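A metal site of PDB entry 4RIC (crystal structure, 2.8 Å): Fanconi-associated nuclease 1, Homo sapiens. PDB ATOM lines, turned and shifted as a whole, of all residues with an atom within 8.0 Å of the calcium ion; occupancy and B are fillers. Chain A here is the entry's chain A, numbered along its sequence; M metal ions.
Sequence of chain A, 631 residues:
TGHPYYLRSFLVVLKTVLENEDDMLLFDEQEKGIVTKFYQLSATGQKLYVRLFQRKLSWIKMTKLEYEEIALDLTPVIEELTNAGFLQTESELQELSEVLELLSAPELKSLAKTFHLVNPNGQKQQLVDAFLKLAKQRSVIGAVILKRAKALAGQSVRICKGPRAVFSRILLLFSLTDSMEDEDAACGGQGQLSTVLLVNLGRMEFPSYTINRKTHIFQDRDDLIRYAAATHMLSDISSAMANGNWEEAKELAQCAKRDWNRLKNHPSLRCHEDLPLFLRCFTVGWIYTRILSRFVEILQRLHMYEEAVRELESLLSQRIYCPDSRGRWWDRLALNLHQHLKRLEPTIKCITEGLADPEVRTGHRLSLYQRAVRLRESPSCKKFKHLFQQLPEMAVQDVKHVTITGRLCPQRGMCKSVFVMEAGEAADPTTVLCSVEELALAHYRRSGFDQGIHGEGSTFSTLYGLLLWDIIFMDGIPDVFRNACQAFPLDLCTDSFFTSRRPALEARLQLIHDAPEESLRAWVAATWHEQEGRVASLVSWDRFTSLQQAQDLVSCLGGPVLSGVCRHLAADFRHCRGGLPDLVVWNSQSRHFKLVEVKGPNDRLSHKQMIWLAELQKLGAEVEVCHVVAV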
ATOM      1  N   VAL A 436       4.081  28.196 -27.762  1.00  0.00           N
ATOM      2  CA  VAL A 436       5.070  28.422 -26.711  1.00  0.00           C
ATOM      3  C   VAL A 436       5.900  29.658 -27.016  1.00  0.00           C
ATOM      4  O   VAL A 436       6.240  30.439 -26.120  1.00  0.00           O
ATOM      5  CB  VAL A 436       6.053  27.246 -26.617  1.00  0.00           C
ATOM      6  CG1 VAL A 436       6.541  27.122 -25.200  1.00  0.00           C
ATOM      7  CG2 VAL A 436       5.392  25.946 -27.067  1.00  0.00           C
ATOM      8  N   GLU A 437       6.218  29.801 -28.302  1.00  0.00           N
ATOM      9  CA  GLU A 437       7.037  30.892 -28.796  1.00  0.00           C
ATOM     10  C   GLU A 437       6.303  32.225 -28.710  1.00  0.00           C
ATOM     11  O   GLU A 437       6.895  33.233 -28.280  1.00  0.00           O
ATOM     12  CB  GLU A 437       7.486  30.601 -30.230  1.00  0.00           C
ATOM     13  CG  GLU A 437       8.485  29.459 -30.341  1.00  0.00           C
ATOM     14  CD  GLU A 437       7.831  28.091 -30.540  1.00  0.00           C
ATOM     15  OE1 GLU A 437       6.587  27.982 -30.404  1.00  0.00           O
ATOM     16  OE2 GLU A 437       8.582  27.120 -30.833  1.00  0.00           O
ATOM     17  N   HIS A 454       9.808  35.354 -34.527  1.00  0.00           N
ATOM     18  CA  HIS A 454       9.984  33.922 -34.373  1.00  0.00           C
ATOM     19  C   HIS A 454      10.310  33.358 -35.745  1.00  0.00           C
ATOM     20  O   HIS A 454       9.418  33.193 -36.572  1.00  0.00           O
ATOM     21  CB  HIS A 454       8.698  33.308 -33.811  1.00  0.00           C
ATOM     22  CG  HIS A 454       8.702  31.819 -33.790  1.00  0.00           C
ATOM     23  ND1 HIS A 454       9.839  31.075 -33.651  1.00  0.00           N
ATOM     24  CD2 HIS A 454       7.676  30.937 -33.866  1.00  0.00           C
ATOM     25  CE1 HIS A 454       9.534  29.794 -33.649  1.00  0.00           C
ATOM     26  NE2 HIS A 454       8.235  29.680 -33.786  1.00  0.00           N
ATOM     27  N   GLU A 456      13.497  31.149 -36.114  1.00  0.00           N
ATOM     28  CA  GLU A 456      14.599  30.188 -35.913  1.00  0.00           C
ATOM     29  C   GLU A 456      15.774  30.497 -36.865  1.00  0.00           C
ATOM     30  O   GLU A 456      16.253  31.629 -36.910  1.00  0.00           O
ATOM     31  CB  GLU A 456      14.096  28.741 -36.022  1.00  0.00           C
ATOM     32  CG  GLU A 456      12.593  28.593 -35.741  1.00  0.00           C
ATOM     33  CD  GLU A 456      12.170  27.263 -35.125  1.00  0.00           C
ATOM     34  OE1 GLU A 456      12.829  26.227 -35.375  1.00  0.00           O
ATOM     35  OE2 GLU A 456      11.133  27.274 -34.396  1.00  0.00           O
ATOM     36  N   LEU A 580      19.940  27.441 -34.540  1.00  0.00           N
ATOM     37  CA  LEU A 580      19.767  28.818 -34.147  1.00  0.00           C
ATOM     38  C   LEU A 580      18.478  28.976 -33.324  1.00  0.00           C
ATOM     39  O   LEU A 580      17.491  28.314 -33.616  1.00  0.00           O
ATOM     40  CB  LEU A 580      19.767  29.701 -35.378  1.00  0.00           C
ATOM     41  CG  LEU A 580      21.144  29.721 -36.052  1.00  0.00           C
ATOM     42  CD1 LEU A 580      20.995  29.944 -37.554  1.00  0.00           C
ATOM     43  CD2 LEU A 580      22.043  30.760 -35.395  1.00  0.00           C
ATOM     44  N   PRO A 581      18.506  29.806 -32.269  1.00  0.00           N
ATOM     45  CA  PRO A 581      17.360  30.060 -31.396  1.00  0.00           C
ATOM     46  C   PRO A 581      16.023  30.339 -32.111  1.00  0.00           C
ATOM     47  O   PRO A 581      16.009  30.831 -33.250  1.00  0.00           O
ATOM     48  CB  PRO A 581      17.782  31.333 -30.655  1.00  0.00           C
ATOM     49  CG  PRO A 581      19.080  31.764 -31.230  1.00  0.00           C
ATOM     50  CD  PRO A 581      19.689  30.561 -31.840  1.00  0.00           C
ATOM     51  N   ASP A 582      14.913  30.033 -31.453  1.00  0.00           N
ATOM     52  CA  ASP A 582      13.596  30.376 -31.952  1.00  0.00           C
ATOM     53  C   ASP A 582      13.410  31.855 -32.238  1.00  0.00           C
ATOM     54  O   ASP A 582      12.783  32.208 -33.238  1.00  0.00           O
ATOM     55  CB  ASP A 582      12.510  29.953 -30.974  1.00  0.00           C
ATOM     56  CG  ASP A 582      12.435  28.445 -30.794  1.00  0.00           C
ATOM     57  OD1 ASP A 582      11.996  27.719 -31.731  1.00  0.00           O
ATOM     58  OD2 ASP A 582      12.811  28.017 -29.693  1.00  0.00           O
ATOM     59  N   LEU A 583      13.964  32.697 -31.376  1.00  0.00           N
ATOM     60  CA  LEU A 583      13.607  34.126 -31.330  1.00  0.00           C
ATOM     61  C   LEU A 583      14.724  35.159 -31.448  1.00  0.00           C
ATOM     62  O   LEU A 583      15.853  34.950 -31.016  1.00  0.00           O
ATOM     63  CB  LEU A 583      12.838  34.394 -30.025  1.00  0.00           C
ATOM     64  CG  LEU A 583      11.315  34.441 -29.992  1.00  0.00           C
ATOM     65  CD1 LEU A 583      10.607  33.309 -30.739  1.00  0.00           C
ATOM     66  CD2 LEU A 583      10.905  34.405 -28.545  1.00  0.00           C
ATOM     67  N   VAL A 596      16.821  34.388 -28.196  1.00  0.00           N
ATOM     68  CA  VAL A 596      16.143  33.546 -27.216  1.00  0.00           C
ATOM     69  C   VAL A 596      15.731  32.213 -27.821  1.00  0.00           C
ATOM     70  O   VAL A 596      15.101  32.180 -28.880  1.00  0.00           O
ATOM     71  CB  VAL A 596      14.875  34.266 -26.706  1.00  0.00           C
ATOM     72  CG1 VAL A 596      14.098  33.411 -25.725  1.00  0.00           C
ATOM     73  CG2 VAL A 596      15.246  35.629 -26.130  1.00  0.00           C
ATOM     74  N   GLU A 597      16.120  31.119 -27.167  1.00  0.00           N
ATOM     75  CA  GLU A 597      15.583  29.803 -27.531  1.00  0.00           C
ATOM     76  C   GLU A 597      14.453  29.455 -26.579  1.00  0.00           C
ATOM     77  O   GLU A 597      14.672  29.334 -25.369  1.00  0.00           O
ATOM     78  CB  GLU A 597      16.667  28.714 -27.488  1.00  0.00           C
ATOM     79  CG  GLU A 597      16.116  27.282 -27.576  1.00  0.00           C
ATOM     80  CD  GLU A 597      15.547  26.918 -28.944  1.00  0.00           C
ATOM     81  OE1 GLU A 597      16.175  27.288 -29.953  1.00  0.00           O
ATOM     82  OE2 GLU A 597      14.461  26.279 -29.032  1.00  0.00           O
ATOM     83  N   VAL A 598      13.260  29.298 -27.123  1.00  0.00           N
ATOM     84  CA  VAL A 598      12.104  28.890 -26.325  1.00  0.00           C
ATOM     85  C   VAL A 598      12.017  27.354 -26.225  1.00  0.00           C
ATOM     86  O   VAL A 598      12.088  26.607 -27.250  1.00  0.00           O
ATOM     87  CB  VAL A 598      10.776  29.466 -26.865  1.00  0.00           C
ATOM     88  CG1 VAL A 598       9.638  29.223 -25.886  1.00  0.00           C
ATOM     89  CG2 VAL A 598      10.902  30.950 -27.119  1.00  0.00           C
ATOM     90  N   LYS A 599      11.877  26.902 -24.972  1.00  0.00           N
ATOM     91  CA  LYS A 599      11.690  25.491 -24.629  1.00  0.00           C
ATOM     92  C   LYS A 599      10.417  25.307 -23.834  1.00  0.00           C
ATOM     93  O   LYS A 599      10.277  25.833 -22.724  1.00  0.00           O
ATOM     94  CB  LYS A 599      12.868  24.945 -23.799  1.00  0.00           C
ATOM     95  CG  LYS A 599      14.208  24.917 -24.513  1.00  0.00           C
ATOM     96  CD  LYS A 599      14.197  23.951 -25.673  1.00  0.00           C
ATOM     97  CE  LYS A 599      15.560  23.838 -26.312  1.00  0.00           C
ATOM     98  NZ  LYS A 599      15.520  22.842 -27.414  1.00  0.00           N
ATOM     99  N   GLY A 600       9.476  24.555 -24.398  1.00  0.00           N
ATOM    100  CA  GLY A 600       8.257  24.179 -23.706  1.00  0.00           C
ATOM    101  C   GLY A 600       8.575  23.208 -22.572  1.00  0.00           C
ATOM    102  O   GLY A 600       9.736  22.860 -22.374  1.00  0.00           O
ATOM    103  N   ASP A 603      10.937  19.799 -23.413  1.00  0.00           N
ATOM    104  CA  ASP A 603      12.070  19.671 -24.308  1.00  0.00           C
ATOM    105  C   ASP A 603      13.291  20.441 -23.823  1.00  0.00           C
ATOM    106  O   ASP A 603      13.149  21.510 -23.236  1.00  0.00           O
ATOM    107  CB  ASP A 603      11.650  19.896 -25.789  1.00  0.00           C
ATOM    108  CG  ASP A 603      12.143  21.209 -26.372  1.00  0.00           C
ATOM    109  OD1 ASP A 603      13.300  21.243 -26.845  1.00  0.00           O
ATOM    110  OD2 ASP A 603      11.365  22.186 -26.398  1.00  0.00           O
ATOM    111  N   ARG A 604      14.466  19.845 -24.004  1.00  0.00           N
ATOM    112  CA  ARG A 604      15.745  20.435 -23.614  1.00  0.00           C
ATOM    113  C   ARG A 604      16.490  20.837 -24.872  1.00  0.00           C
ATOM    114  O   ARG A 604      16.020  20.591 -25.982  1.00  0.00           O
ATOM    115  CB  ARG A 604      16.594  19.434 -22.832  1.00  0.00           C
ATOM    116  CG  ARG A 604      15.935  18.861 -21.583  1.00  0.00           C
ATOM    117  CD  ARG A 604      16.898  18.063 -20.703  1.00  0.00           C
ATOM    118  NE  ARG A 604      17.614  17.011 -21.443  1.00  0.00           N
ATOM    119  CZ  ARG A 604      18.915  17.023 -21.697  1.00  0.00           C
ATOM    120  NH1 ARG A 604      19.672  18.019 -21.275  1.00  0.00           N
ATOM    121  NH2 ARG A 604      19.467  16.020 -22.380  1.00  0.00           N
ATOM    122  N   LEU A 605      17.646  21.459 -24.703  1.00  0.00           N
ATOM    123  CA  LEU A 605      18.486  21.834 -25.806  1.00  0.00           C
ATOM    124  C   LEU A 605      19.100  20.607 -26.490  1.00  0.00           C
ATOM    125  O   LEU A 605      19.587  19.697 -25.839  1.00  0.00           O
ATOM    126  CB  LEU A 605      19.630  22.708 -25.338  1.00  0.00           C
ATOM    127  CG  LEU A 605      19.508  23.944 -24.473  1.00  0.00           C
ATOM    128  CD1 LEU A 605      20.907  24.403 -24.117  1.00  0.00           C
ATOM    129  CD2 LEU A 605      18.785  25.053 -25.200  1.00  0.00           C
ATOM    130  N   GLN A 609      21.882  23.196 -30.788  1.00  0.00           N
ATOM    131  CA  GLN A 609      21.433  24.410 -30.162  1.00  0.00           C
ATOM    132  C   GLN A 609      22.422  24.927 -29.161  1.00  0.00           C
ATOM    133  O   GLN A 609      22.633  26.137 -29.113  1.00  0.00           O
ATOM    134  CB  GLN A 609      20.109  24.215 -29.473  1.00  0.00           C
ATOM    135  CG  GLN A 609      18.960  24.252 -30.454  1.00  0.00           C
ATOM    136  CD  GLN A 609      17.697  23.692 -29.852  1.00  0.00           C
ATOM    137  OE1 GLN A 609      17.737  22.861 -28.940  1.00  0.00           O
ATOM    138  NE2 GLN A 609      16.567  24.141 -30.355  1.00  0.00           N
ATOM    139  N   CYS A 626      14.555  30.185 -22.610  1.00  0.00           N
ATOM    140  CA  CYS A 626      13.311  30.598 -21.968  1.00  0.00           C
ATOM    141  C   CYS A 626      12.339  29.423 -21.860  1.00  0.00           C
ATOM    142  O   CYS A 626      11.737  29.005 -22.847  1.00  0.00           O
ATOM    143  CB  CYS A 626      12.701  31.784 -22.713  1.00  0.00           C
ATOM    144  SG  CYS A 626      11.021  32.245 -22.238  1.00  0.00           S
HETATM  145 CA    CA M   1      12.222  25.816 -29.434  1.00  0.00          CA
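NZ of Lys 599 lies close to OE2 of Glu 597 (3.9 Å).
O of Asp 582 is in hydrogen-bond range of N of Glu 456 (3.1 Å).
O of Asp 582 lies within hydrogen-bond range of ND1 of His 454 (3.2 Å).
The backbone NH (N) of Cys 626 sits at hydrogen-bond distance from the backbone carbonyl oxygen (O) of Glu 597, 2.9 Å away.
OE1 of Glu 597 lies within hydrogen-bond range of NE2 of Gln 609 (3.2 Å).
The backbone carbonyl oxygen of Val 596 lies within hydrogen-bond range of the backbone NH of Asp 582 (3.4 Å).
Three residues have an atom within 4 Å of the calcium ion: Asp 582, Glu 597 and Val 598.
The nearest printed residue that does not touch the calcium ion is Glu 437 (4.1 Å).
The side-chain carboxylate (OD2) of Asp 582 binds the calcium ion (2.3 Å).
OE2 of Glu 597 binds the calcium ion.
The calcium ion is bound by O of Val 598, at 2.3 Å.
Slightly farther from the calcium ion lies OD1 of Asp 582 (3.0 Å).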
